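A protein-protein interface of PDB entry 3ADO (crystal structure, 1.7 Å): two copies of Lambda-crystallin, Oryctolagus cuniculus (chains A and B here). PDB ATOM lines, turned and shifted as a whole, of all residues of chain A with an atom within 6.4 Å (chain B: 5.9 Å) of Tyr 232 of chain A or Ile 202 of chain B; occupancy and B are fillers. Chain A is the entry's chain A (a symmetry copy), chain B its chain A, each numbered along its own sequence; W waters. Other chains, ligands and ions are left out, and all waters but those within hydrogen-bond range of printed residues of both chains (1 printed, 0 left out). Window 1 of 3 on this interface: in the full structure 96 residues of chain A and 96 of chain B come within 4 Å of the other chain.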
ATOM      1  N   LEU A 198      27.082   8.109  24.846  1.00  0.00           N
ATOM      2  CA  LEU A 198      25.993   9.049  24.638  1.00  0.00           C
ATOM      3  C   LEU A 198      26.498  10.467  24.891  1.00  0.00           C
ATOM      4  O   LEU A 198      26.174  11.388  24.144  1.00  0.00           O
ATOM      5  CB  LEU A 198      24.816   8.741  25.574  1.00  0.00           C
ATOM      6  CG  LEU A 198      24.120   7.387  25.399  1.00  0.00           C
ATOM      7  CD1 LEU A 198      22.980   7.276  26.411  1.00  0.00           C
ATOM      8  CD2 LEU A 198      23.584   7.250  23.973  1.00  0.00           C
ATOM      9  N   ALA A 201      28.520  11.724  21.992  1.00  0.00           N
ATOM     10  CA  ALA A 201      27.674  11.959  20.819  1.00  0.00           C
ATOM     11  C   ALA A 201      27.117  13.380  20.891  1.00  0.00           C
ATOM     12  O   ALA A 201      27.054  14.089  19.885  1.00  0.00           O
ATOM     13  CB  ALA A 201      26.520  10.938  20.771  1.00  0.00           C
ATOM     14  N   ILE A 202      26.714  13.787  22.091  1.00  0.00           N
ATOM     15  CA  ILE A 202      26.170  15.118  22.313  1.00  0.00           C
ATOM     16  C   ILE A 202      27.239  16.184  22.150  1.00  0.00           C
ATOM     17  O   ILE A 202      27.030  17.190  21.467  1.00  0.00           O
ATOM     18  CB  ILE A 202      25.572  15.245  23.738  1.00  0.00           C
ATOM     19  CG1 ILE A 202      24.370  14.316  23.873  1.00  0.00           C
ATOM     20  CG2 ILE A 202      25.178  16.695  24.014  1.00  0.00           C
ATOM     21  CD1 ILE A 202      23.858  14.174  25.301  1.00  0.00           C
ATOM     22  N   MET A 224      20.090  22.724  26.535  1.00  0.00           N
ATOM     23  CA  MET A 224      20.030  21.487  27.295  1.00  0.00           C
ATOM     24  C   MET A 224      19.457  21.694  28.704  1.00  0.00           C
ATOM     25  O   MET A 224      18.437  21.099  29.042  1.00  0.00           O
ATOM     26  CB  MET A 224      21.420  20.843  27.399  1.00  0.00           C
ATOM     27  CG  MET A 224      21.445  19.509  28.140  1.00  0.00           C
ATOM     28  SD  MET A 224      20.609  18.164  27.272  1.00  0.00           S
ATOM     29  CE  MET A 224      21.930  17.605  26.174  1.00  0.00           C
ATOM     30  N   GLY A 227      15.955  23.001  28.613  1.00  0.00           N
ATOM     31  CA  GLY A 227      15.162  22.381  27.565  1.00  0.00           C
ATOM     32  C   GLY A 227      15.192  20.864  27.526  1.00  0.00           C
ATOM     33  O   GLY A 227      14.520  20.198  28.315  1.00  0.00           O
ATOM     34  N   LEU A 228      15.979  20.317  26.604  1.00  0.00           N
ATOM     35  CA  LEU A 228      16.073  18.871  26.425  1.00  0.00           C
ATOM     36  C   LEU A 228      16.494  18.109  27.680  1.00  0.00           C
ATOM     37  O   LEU A 228      15.995  17.015  27.944  1.00  0.00           O
ATOM     38  CB  LEU A 228      17.047  18.558  25.280  1.00  0.00           C
ATOM     39  CG  LEU A 228      17.187  17.092  24.854  1.00  0.00           C
ATOM     40  CD1 LEU A 228      15.852  16.567  24.348  1.00  0.00           C
ATOM     41  CD2 LEU A 228      18.241  16.979  23.757  1.00  0.00           C
ATOM     42  N   GLY A 229      17.402  18.693  28.452  1.00  0.00           N
ATOM     43  CA  GLY A 229      17.886  18.034  29.655  1.00  0.00           C
ATOM     44  C   GLY A 229      16.844  17.814  30.734  1.00  0.00           C
ATOM     45  O   GLY A 229      16.962  16.886  31.534  1.00  0.00           O
ATOM     46  N   MET A 230      15.814  18.652  30.764  1.00  0.00           N
ATOM     47  CA  MET A 230      14.782  18.511  31.785  1.00  0.00           C
ATOM     48  C   MET A 230      14.012  17.202  31.637  1.00  0.00           C
ATOM     49  O   MET A 230      13.696  16.541  32.628  1.00  0.00           O
ATOM     50  CB  MET A 230      13.839  19.712  31.745  1.00  0.00           C
ATOM     51  CG  MET A 230      14.524  21.000  32.176  1.00  0.00           C
ATOM     52  SD  MET A 230      13.414  22.418  32.226  1.00  0.00           S
ATOM     53  CE  MET A 230      12.261  21.920  33.493  1.00  0.00           C
ATOM     54  N   ARG A 231      13.714  16.812  30.404  1.00  0.00           N
ATOM     55  CA  ARG A 231      12.998  15.559  30.208  1.00  0.00           C
ATOM     56  C   ARG A 231      13.917  14.381  30.536  1.00  0.00           C
ATOM     57  O   ARG A 231      13.483  13.385  31.120  1.00  0.00           O
ATOM     58  CB  ARG A 231      12.504  15.438  28.761  1.00  0.00           C
ATOM     59  CG  ARG A 231      13.561  15.007  27.764  1.00  0.00           C
ATOM     60  CD  ARG A 231      13.024  15.071  26.339  1.00  0.00           C
ATOM     61  NE  ARG A 231      12.667  16.438  25.965  1.00  0.00           N
ATOM     62  CZ  ARG A 231      12.332  16.822  24.735  1.00  0.00           C
ATOM     63  NH1 ARG A 231      12.302  15.944  23.738  1.00  0.00           N
ATOM     64  NH2 ARG A 231      12.046  18.094  24.499  1.00  0.00           N
ATOM     65  N   TYR A 232      15.191  14.511  30.173  1.00  0.00           N
ATOM     66  CA  TYR A 232      16.166  13.447  30.397  1.00  0.00           C
ATOM     67  C   TYR A 232      16.490  13.134  31.853  1.00  0.00           C
ATOM     68  O   TYR A 232      17.111  12.115  32.152  1.00  0.00           O
ATOM     69  CB  TYR A 232      17.460  13.750  29.631  1.00  0.00           C
ATOM     70  CG  TYR A 232      17.335  13.587  28.128  1.00  0.00           C
ATOM     71  CD1 TYR A 232      16.293  12.844  27.567  1.00  0.00           C
ATOM     72  CD2 TYR A 232      18.284  14.139  27.267  1.00  0.00           C
ATOM     73  CE1 TYR A 232      16.205  12.651  26.184  1.00  0.00           C
ATOM     74  CE2 TYR A 232      18.204  13.954  25.889  1.00  0.00           C
ATOM     75  CZ  TYR A 232      17.167  13.210  25.355  1.00  0.00           C
ATOM     76  OH  TYR A 232      17.119  13.011  23.995  1.00  0.00           O
ATOM     77  N   ALA A 233      16.075  14.002  32.763  1.00  0.00           N
ATOM     78  CA  ALA A 233      16.322  13.760  34.175  1.00  0.00           C
ATOM     79  C   ALA A 233      15.300  12.753  34.696  1.00  0.00           C
ATOM     80  O   ALA A 233      15.454  12.218  35.792  1.00  0.00           O
ATOM     81  CB  ALA A 233      16.211  15.060  34.952  1.00  0.00           C
ATOM     82  N   PHE A 234      14.264  12.489  33.900  1.00  0.00           N
ATOM     83  CA  PHE A 234      13.205  11.567  34.300  1.00  0.00           C
ATOM     84  C   PHE A 234      12.964  10.412  33.344  1.00  0.00           C
ATOM     85  O   PHE A 234      12.608   9.312  33.770  1.00  0.00           O
ATOM     86  CB  PHE A 234      11.890  12.330  34.456  1.00  0.00           C
ATOM     87  CG  PHE A 234      11.957  13.435  35.452  1.00  0.00           C
ATOM     88  CD1 PHE A 234      12.018  13.157  36.811  1.00  0.00           C
ATOM     89  CD2 PHE A 234      11.985  14.760  35.035  1.00  0.00           C
ATOM     90  CE1 PHE A 234      12.108  14.184  37.739  1.00  0.00           C
ATOM     91  CE2 PHE A 234      12.074  15.791  35.959  1.00  0.00           C
ATOM     92  CZ  PHE A 234      12.135  15.503  37.312  1.00  0.00           C
ATOM     93  N   ILE A 235      13.130  10.674  32.053  1.00  0.00           N
ATOM     94  CA  ILE A 235      12.896   9.661  31.031  1.00  0.00           C
ATOM     95  C   ILE A 235      14.006   9.651  29.991  1.00  0.00           C
ATOM     96  O   ILE A 235      14.503  10.704  29.602  1.00  0.00           O
ATOM     97  CB  ILE A 235      11.548   9.916  30.330  1.00  0.00           C
ATOM     98  CG1 ILE A 235      10.414   9.838  31.359  1.00  0.00           C
ATOM     99  CG2 ILE A 235      11.323   8.896  29.226  1.00  0.00           C
ATOM    100  CD1 ILE A 235       9.054  10.190  30.804  1.00  0.00           C
ATOM    101  N   GLY A 236      14.379   8.452  29.548  1.00  0.00           N
ATOM    102  CA  GLY A 236      15.434   8.303  28.559  1.00  0.00           C
ATOM    103  C   GLY A 236      15.069   8.771  27.162  1.00  0.00           C
ATOM    104  O   GLY A 236      13.921   9.131  26.901  1.00  0.00           O
ATOM    105  N   PRO A 237      16.029   8.750  26.226  1.00  0.00           N
ATOM    106  CA  PRO A 237      15.776   9.192  24.849  1.00  0.00           C
ATOM    107  C   PRO A 237      14.790   8.353  24.042  1.00  0.00           C
ATOM    108  O   PRO A 237      14.108   8.879  23.167  1.00  0.00           O
ATOM    109  CB  PRO A 237      17.174   9.209  24.232  1.00  0.00           C
ATOM    110  CG  PRO A 237      17.869   8.099  24.954  1.00  0.00           C
ATOM    111  CD  PRO A 237      17.422   8.295  26.388  1.00  0.00           C
ATOM    112  N   LEU A 238      14.713   7.056  24.335  1.00  0.00           N
ATOM    113  CA  LEU A 238      13.800   6.182  23.606  1.00  0.00           C
ATOM    114  C   LEU A 238      12.372   6.342  24.110  1.00  0.00           C
ATOM    115  O   LEU A 238      11.445   6.509  23.315  1.00  0.00           O
ATOM    116  CB  LEU A 238      14.253   4.723  23.725  1.00  0.00           C
ATOM    117  CG  LEU A 238      15.678   4.473  23.219  1.00  0.00           C
ATOM    118  CD1 LEU A 238      16.037   2.998  23.370  1.00  0.00           C
ATOM    119  CD2 LEU A 238      15.787   4.917  21.759  1.00  0.00           C
ATOM    120  N   THR A 240      11.296   8.808  25.518  1.00  0.00           N
ATOM    121  CA  THR A 240      10.955  10.188  25.186  1.00  0.00           C
ATOM    122  C   THR A 240      10.296  10.219  23.808  1.00  0.00           C
ATOM    123  O   THR A 240       9.304  10.917  23.600  1.00  0.00           O
ATOM    124  CB  THR A 240      12.211  11.092  25.189  1.00  0.00           C
ATOM    125  OG1 THR A 240      12.611  11.339  26.540  1.00  0.00           O
ATOM    126  CG2 THR A 240      11.933  12.418  24.493  1.00  0.00           C
ATOM    127  N   LEU A 263      20.821  14.106  10.509  1.00  0.00           N
ATOM    128  CA  LEU A 263      22.034  13.349  10.799  1.00  0.00           C
ATOM    129  C   LEU A 263      22.987  13.326   9.606  1.00  0.00           C
ATOM    130  O   LEU A 263      24.207  13.375   9.770  1.00  0.00           O
ATOM    131  CB  LEU A 263      21.661  11.925  11.229  1.00  0.00           C
ATOM    132  CG  LEU A 263      20.957  11.859  12.594  1.00  0.00           C
ATOM    133  CD1 LEU A 263      20.395  10.467  12.842  1.00  0.00           C
ATOM    134  CD2 LEU A 263      21.945  12.240  13.688  1.00  0.00           C
ATOM    135  N   LYS A 313      13.097  12.638  42.423  1.00  0.00           N
ATOM    136  CA  LYS A 313      12.954  11.444  41.607  1.00  0.00           C
ATOM    137  C   LYS A 313      12.388  10.289  42.427  1.00  0.00           C
ATOM    138  O   LYS A 313      11.511   9.555  41.992  1.00  0.00           O
ATOM    139  CB  LYS A 313      14.332  11.071  41.062  1.00  0.00           C
ATOM    140  CG  LYS A 313      14.693  11.862  39.803  1.00  0.00           C
ATOM    141  CD  LYS A 313      16.101  11.539  39.298  1.00  0.00           C
ATOM    142  CE  LYS A 313      16.217  10.108  38.762  1.00  0.00           C
ATOM    143  NZ  LYS A 313      15.567  10.019  37.456  1.00  0.00           N
ATOM    144  N   ARG B 197      18.748  18.838  16.901  1.00  0.00           N
ATOM    145  CA  ARG B 197      20.020  18.328  16.416  1.00  0.00           C
ATOM    146  C   ARG B 197      20.712  17.576  17.550  1.00  0.00           C
ATOM    147  O   ARG B 197      21.284  16.510  17.339  1.00  0.00           O
ATOM    148  CB  ARG B 197      20.897  19.467  15.879  1.00  0.00           C
ATOM    149  CG  ARG B 197      20.352  20.077  14.585  1.00  0.00           C
ATOM    150  CD  ARG B 197      21.331  21.060  13.948  1.00  0.00           C
ATOM    151  NE  ARG B 197      22.455  20.406  13.276  1.00  0.00           N
ATOM    152  CZ  ARG B 197      22.456  20.022  12.000  1.00  0.00           C
ATOM    153  NH1 ARG B 197      21.389  20.222  11.241  1.00  0.00           N
ATOM    154  NH2 ARG B 197      23.536  19.453  11.477  1.00  0.00           N
ATOM    155  N   LEU B 198      20.653  18.116  18.765  1.00  0.00           N
ATOM    156  CA  LEU B 198      21.265  17.425  19.888  1.00  0.00           C
ATOM    157  C   LEU B 198      20.468  16.160  20.194  1.00  0.00           C
ATOM    158  O   LEU B 198      21.046  15.106  20.455  1.00  0.00           O
ATOM    159  CB  LEU B 198      21.306  18.327  21.129  1.00  0.00           C
ATOM    160  CG  LEU B 198      22.142  19.608  21.035  1.00  0.00           C
ATOM    161  CD1 LEU B 198      22.061  20.357  22.366  1.00  0.00           C
ATOM    162  CD2 LEU B 198      23.595  19.265  20.703  1.00  0.00           C
ATOM    163  N   GLN B 199      19.140  16.258  20.153  1.00  0.00           N
ATOM    164  CA  GLN B 199      18.311  15.092  20.443  1.00  0.00           C
ATOM    165  C   GLN B 199      18.564  13.951  19.462  1.00  0.00           C
ATOM    166  O   GLN B 199      18.688  12.790  19.863  1.00  0.00           O
ATOM    167  CB  GLN B 199      16.819  15.446  20.423  1.00  0.00           C
ATOM    168  CG  GLN B 199      15.957  14.295  20.950  1.00  0.00           C
ATOM    169  CD  GLN B 199      14.463  14.572  20.957  1.00  0.00           C
ATOM    170  OE1 GLN B 199      13.701  13.835  21.587  1.00  0.00           O
ATOM    171  NE2 GLN B 199      14.033  15.618  20.250  1.00  0.00           N
ATOM    172  N   TYR B 200      18.643  14.280  18.176  1.00  0.00           N
ATOM    173  CA  TYR B 200      18.876  13.265  17.157  1.00  0.00           C
ATOM    174  C   TYR B 200      20.271  12.651  17.277  1.00  0.00           C
ATOM    175  O   TYR B 200      20.457  11.476  16.972  1.00  0.00           O
ATOM    176  CB  TYR B 200      18.674  13.852  15.756  1.00  0.00           C
ATOM    177  CG  TYR B 200      17.245  14.281  15.447  1.00  0.00           C
ATOM    178  CD1 TYR B 200      16.187  13.961  16.304  1.00  0.00           C
ATOM    179  CD2 TYR B 200      16.958  15.008  14.291  1.00  0.00           C
ATOM    180  CE1 TYR B 200      14.879  14.362  16.014  1.00  0.00           C
ATOM    181  CE2 TYR B 200      15.658  15.409  13.991  1.00  0.00           C
ATOM    182  CZ  TYR B 200      14.624  15.085  14.855  1.00  0.00           C
ATOM    183  OH  TYR B 200      13.341  15.491  14.552  1.00  0.00           O
ATOM    184  N   ALA B 201      21.245  13.440  17.729  1.00  0.00           N
ATOM    185  CA  ALA B 201      22.608  12.935  17.911  1.00  0.00           C
ATOM    186  C   ALA B 201      22.584  11.818  18.952  1.00  0.00           C
ATOM    187  O   ALA B 201      23.250  10.793  18.800  1.00  0.00           O
ATOM    188  CB  ALA B 201      23.548  14.068  18.368  1.00  0.00           C
ATOM    189  N   ILE B 202      21.808  12.027  20.012  1.00  0.00           N
ATOM    190  CA  ILE B 202      21.679  11.048  21.081  1.00  0.00           C
ATOM    191  C   ILE B 202      20.942   9.807  20.604  1.00  0.00           C
ATOM    192  O   ILE B 202      21.384   8.680  20.841  1.00  0.00           O
ATOM    193  CB  ILE B 202      20.904  11.638  22.286  1.00  0.00           C
ATOM    194  CG1 ILE B 202      21.712  12.773  22.908  1.00  0.00           C
ATOM    195  CG2 ILE B 202      20.618  10.543  23.313  1.00  0.00           C
ATOM    196  CD1 ILE B 202      20.941  13.585  23.940  1.00  0.00           C
ATOM    197  N   ILE B 203      19.812  10.019  19.937  1.00  0.00           N
ATOM    198  CA  ILE B 203      19.002   8.914  19.440  1.00  0.00           C
ATOM    199  C   ILE B 203      19.787   8.021  18.474  1.00  0.00           C
ATOM    200  O   ILE B 203      19.710   6.790  18.553  1.00  0.00           O
ATOM    201  CB  ILE B 203      17.726   9.447  18.737  1.00  0.00           C
ATOM    202  CG1 ILE B 203      16.776  10.058  19.777  1.00  0.00           C
ATOM    203  CG2 ILE B 203      17.030   8.319  17.984  1.00  0.00           C
ATOM    204  CD1 ILE B 203      15.610  10.836  19.179  1.00  0.00           C
ATOM    205  N   SER B 204      20.545   8.639  17.573  1.00  0.00           N
ATOM    206  CA  SER B 204      21.333   7.887  16.597  1.00  0.00           C
ATOM    207  C   SER B 204      22.279   6.881  17.261  1.00  0.00           C
ATOM    208  O   SER B 204      22.305   5.706  16.888  1.00  0.00           O
ATOM    209  CB  SER B 204      22.140   8.842  15.710  1.00  0.00           C
ATOM    210  OG  SER B 204      22.743   8.133  14.637  1.00  0.00           O
ATOM    211  N   GLU B 205      23.054   7.337  18.243  1.00  0.00           N
ATOM    212  CA  GLU B 205      23.991   6.451  18.943  1.00  0.00           C
ATOM    213  C   GLU B 205      23.241   5.453  19.831  1.00  0.00           C
ATOM    214  O   GLU B 205      23.614   4.283  19.920  1.00  0.00           O
ATOM    215  CB  GLU B 205      24.981   7.289  19.770  1.00  0.00           C
ATOM    216  CG  GLU B 205      25.902   6.511  20.712  1.00  0.00           C
ATOM    217  CD  GLU B 205      26.749   5.456  20.015  1.00  0.00           C
ATOM    218  OE1 GLU B 205      26.868   5.485  18.771  1.00  0.00           O
ATOM    219  OE2 GLU B 205      27.313   4.594  20.726  1.00  0.00           O
ATOM    220  N   ALA B 206      22.174   5.906  20.480  1.00  0.00           N
ATOM    221  CA  ALA B 206      21.390   5.018  21.328  1.00  0.00           C
ATOM    222  C   ALA B 206      20.836   3.870  20.481  1.00  0.00           C
ATOM    223  O   ALA B 206      20.858   2.707  20.884  1.00  0.00           O
ATOM    224  CB  ALA B 206      20.242   5.788  21.976  1.00  0.00           C
ATOM    225  N   TRP B 207      20.346   4.212  19.295  1.00  0.00           N
ATOM    226  CA  TRP B 207      19.771   3.218  18.393  1.00  0.00           C
ATOM    227  C   TRP B 207      20.786   2.135  18.045  1.00  0.00           C
ATOM    228  O   TRP B 207      20.473   0.944  18.085  1.00  0.00           O
ATOM    229  CB  TRP B 207      19.279   3.904  17.120  1.00  0.00           C
ATOM    230  CG  TRP B 207      18.197   3.160  16.407  1.00  0.00           C
ATOM    231  CD1 TRP B 207      18.339   2.312  15.341  1.00  0.00           C
ATOM    232  CD2 TRP B 207      16.797   3.204  16.703  1.00  0.00           C
ATOM    233  NE1 TRP B 207      17.109   1.829  14.956  1.00  0.00           N
ATOM    234  CE2 TRP B 207      16.145   2.360  15.774  1.00  0.00           C
ATOM    235  CE3 TRP B 207      16.028   3.877  17.663  1.00  0.00           C
ATOM    236  CZ2 TRP B 207      14.759   2.170  15.778  1.00  0.00           C
ATOM    237  CZ3 TRP B 207      14.646   3.688  17.667  1.00  0.00           C
ATOM    238  CH2 TRP B 207      14.028   2.839  16.726  1.00  0.00           C
ATOM    239  N   MET B 224      20.423   7.275  30.920  1.00  0.00           N
ATOM    240  CA  MET B 224      20.131   8.696  30.835  1.00  0.00           C
ATOM    241  C   MET B 224      19.337   9.204  32.047  1.00  0.00           C
ATOM    242  O   MET B 224      19.808  10.085  32.760  1.00  0.00           O
ATOM    243  CB  MET B 224      19.358   9.018  29.547  1.00  0.00           C
ATOM    244  CG  MET B 224      19.051  10.500  29.348  1.00  0.00           C
ATOM    245  SD  MET B 224      20.506  11.521  29.030  1.00  0.00           S
ATOM    246  CE  MET B 224      20.688  11.294  27.247  1.00  0.00           C
ATOM    247  N   SER B 225      18.157   8.631  32.298  1.00  0.00           N
ATOM    248  CA  SER B 225      17.299   9.101  33.391  1.00  0.00           C
ATOM    249  C   SER B 225      17.876   9.020  34.802  1.00  0.00           C
ATOM    250  O   SER B 225      17.596   9.880  35.640  1.00  0.00           O
ATOM    251  CB  SER B 225      15.936   8.389  33.361  1.00  0.00           C
ATOM    252  OG  SER B 225      16.051   6.999  33.619  1.00  0.00           O
ATOM    253  N   ASP B 226      18.674   7.995  35.068  1.00  0.00           N
ATOM    254  CA  ASP B 226      19.273   7.849  36.386  1.00  0.00           C
ATOM    255  C   ASP B 226      20.768   8.129  36.336  1.00  0.00           C
ATOM    256  O   ASP B 226      21.493   7.806  37.274  1.00  0.00           O
ATOM    257  CB  ASP B 226      19.036   6.439  36.926  1.00  0.00           C
ATOM    258  CG  ASP B 226      17.665   6.277  37.553  1.00  0.00           C
ATOM    259  OD1 ASP B 226      16.927   7.278  37.642  1.00  0.00           O
ATOM    260  OD2 ASP B 226      17.333   5.149  37.966  1.00  0.00           O
ATOM    261  N   LEU B 228      23.327  10.313  33.165  1.00  0.00           N
ATOM    262  CA  LEU B 228      23.716  11.507  32.420  1.00  0.00           C
ATOM    263  C   LEU B 228      22.653  12.604  32.394  1.00  0.00           C
ATOM    264  O   LEU B 228      22.977  13.790  32.465  1.00  0.00           O
ATOM    265  CB  LEU B 228      24.088  11.116  30.982  1.00  0.00           C
ATOM    266  CG  LEU B 228      24.645  12.218  30.073  1.00  0.00           C
ATOM    267  CD1 LEU B 228      25.944  12.762  30.650  1.00  0.00           C
ATOM    268  CD2 LEU B 228      24.890  11.652  28.679  1.00  0.00           C
ATOM    269  N   GLY B 229      21.390  12.206  32.302  1.00  0.00           N
ATOM    270  CA  GLY B 229      20.309  13.176  32.243  1.00  0.00           C
ATOM    271  C   GLY B 229      20.140  14.030  33.486  1.00  0.00           C
ATOM    272  O   GLY B 229      19.646  15.154  33.406  1.00  0.00           O
ATOM    273  N   MET B 230      20.554  13.513  34.637  1.00  0.00           N
ATOM    274  CA  MET B 230      20.408  14.271  35.875  1.00  0.00           C
ATOM    275  C   MET B 230      21.258  15.538  35.870  1.00  0.00           C
ATOM    276  O   MET B 230      20.818  16.594  36.329  1.00  0.00           O
ATOM    277  CB  MET B 230      20.746  13.385  37.073  1.00  0.00           C
ATOM    278  CG  MET B 230      19.733  12.270  37.273  1.00  0.00           C
ATOM    279  SD  MET B 230      20.056  11.263  38.732  1.00  0.00           S
ATOM    280  CE  MET B 230      19.866  12.462  40.039  1.00  0.00           C
ATOM    281  N   TYR B 232      22.259  17.090  33.156  1.00  0.00           N
ATOM    282  CA  TYR B 232      21.728  17.921  32.079  1.00  0.00           C
ATOM    283  C   TYR B 232      20.473  18.721  32.408  1.00  0.00           C
ATOM    284  O   TYR B 232      20.086  19.617  31.659  1.00  0.00           O
ATOM    285  CB  TYR B 232      21.487  17.068  30.827  1.00  0.00           C
ATOM    286  CG  TYR B 232      22.761  16.631  30.128  1.00  0.00           C
ATOM    287  CD1 TYR B 232      23.973  17.285  30.362  1.00  0.00           C
ATOM    288  CD2 TYR B 232      22.745  15.591  29.198  1.00  0.00           C
ATOM    289  CE1 TYR B 232      25.138  16.915  29.682  1.00  0.00           C
ATOM    290  CE2 TYR B 232      23.900  15.214  28.517  1.00  0.00           C
ATOM    291  CZ  TYR B 232      25.088  15.879  28.760  1.00  0.00           C
ATOM    292  OH  TYR B 232      26.213  15.515  28.056  1.00  0.00           O
HETATM  293  O   HOH W   1      15.026  11.735  22.844  1.00  0.00           O
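Water W1 lies within hydrogen-bond range of the side-chain hydroxyl (OH) of Tyr 232 of chain A (2.7 Å), the side-chain amide oxygen (OE1) of Gln 199 of chain B (2.8 Å) and the backbone carbonyl oxygen (O) of Pro 237 of chain A (3.0 Å).
Ala 201 of chain A touches Ala 201 of chain B (O to CB, 3.8 Å).
Ile 202 of chain B touches Ile 202 of chain A (CG1 to CG1, 3.2 Å).
CD2 of Leu 228 of chain A touches N of Gln 199 of chain B (3.8 Å).
Gly 229 of chain A touches Gly 229 of chain B (O to O, 3.7 Å).
Tyr 232 of chain A touches Gly 229 of chain B (O to CA, 3.4 Å).
Ile 235 of chain A touches Ser 225 of chain B.
CB of Pro 237 of chain A touches CG2 of Ile 202 of chain B, 3.8 Å away.
CB of Met 224 of chain B touches CD of Pro 237 of chain A (3.8 Å).
O of Tyr 200 of chain B touches CD2 of Leu 263 of chain A, 3.7 Å away.
Leu 263 of chain A touches Ser 204 of chain B (CD1 to CB, 3.7 Å).
O of Tyr 232 of chain A lies close to O of Met 224 of chain B (3.4 Å).
The side-chain carboxylate (OD1) of Asp 226 of chain B lies within salt-bridge range of the side-chain amino group (NZ) of Lys 313 of chain A, 3.1 Å away.
OE1 of Gln 199 of chain B is in hydrogen-bond range of NH1 of Arg 231 of chain A, 3.3 Å away.
The backbone carbonyl oxygen (O) of Ser 225 of chain B is in hydrogen-bond range of the side-chain amino group (NZ) of Lys 313 of chain A (2.7 Å).
O of Ser 225 of chain B sits close to O of Ala 233 of chain A (3.2 Å).
The backbone carbonyl oxygen (O) of Met 224 of chain A sits close to the backbone carbonyl oxygen (O) of Tyr 232 of chain B, 3.4 Å away.
Ile 202 of chain A touches Tyr 232 of chain B, and with the chains exchanged Tyr 232 of chain A touches Ile 202 of chain B.
Met 224 of chain A touches Tyr 232 of chain B, and with the chains exchanged Tyr 232 of chain A touches Met 224 of chain B.
Gly 229 of chain A touches its own counterpart, Gly 229 of chain B.
Gly 229 of chain A touches Tyr 232 of chain B, and with the chains exchanged Tyr 232 of chain A touches Gly 229 of chain B.
Positions printed for both chains: 198, 201, 202, 224, 228, 229, 230 and 232.
Of the 26 pairs that touch across the chains among the printed residues, 9 have their exchanged pair printed and touching as well.
Of the printed residues of chain B, Tyr 232 of chain A touches Gln 199 (3.5 Å), Ile 202 (3.4 Å), Met 224 (3.4 Å), Ser 225 (3.3 Å) and Gly 229 (3.4 Å).
Printed residues of chain B within 4 Å of Met 224 of chain A: Tyr 232 (3.4 Å).
Printed residues of chain B within 4 Å of Ile 235 of chain A: Ser 225.
Of the printed residues of chain B, Leu 263 of chain A touches Tyr 200 (3.7 Å) and Ser 204 (3.7 Å).
Printed residues of chain A within 4 Å of Met 230 of chain B: Lys 313 (3.9 Å).
Leu 238 of chain A touches none of the printed residues of chain B.
Gly 236 of chain A touches none of the printed residues of chain B.
The nearest printed residue of chain B that does not touch Ala 201 of chain A is Glu 205 of chain B (4.1 Å).
Of the 19 printed residues of chain A, 15 touch a printed residue of chain B.
Hydrophobic or aromatic side chains of chain A that line the printed part of chain B: Leu 198, Ala 201, Ile 202, Met 224, Leu 228, Tyr 232, Ala 233, Pro 237 and Leu 263.
Of the 18 printed residues of chain B, 12 touch a printed residue of chain A.
Hydrophobic or aromatic side chains of chain B that line the printed part of chain A: Ala 201, Ile 202, Met 224, Met 230 and Tyr 232.
Along chain B the printed residues that touch a printed residue of chain A span positions 199 to 232.
OG1 of Thr 240 of chain A sits at hydrogen-bond distance from O of Gly 236 of chain A (2.6 Å).
The backbone carbonyl oxygen of Met 224 of chain A lies within hydrogen-bond range of the backbone NH of Gly 229 of chain A (2.7 Å).
NZ of Lys 313 of chain A sits at hydrogen-bond distance from O of Ala 233 of chain A, 2.8 Å away.
The backbone NH of Gly 229 of chain B is in hydrogen-bond range of the backbone carbonyl oxygen of Met 224 of chain B (2.7 Å).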
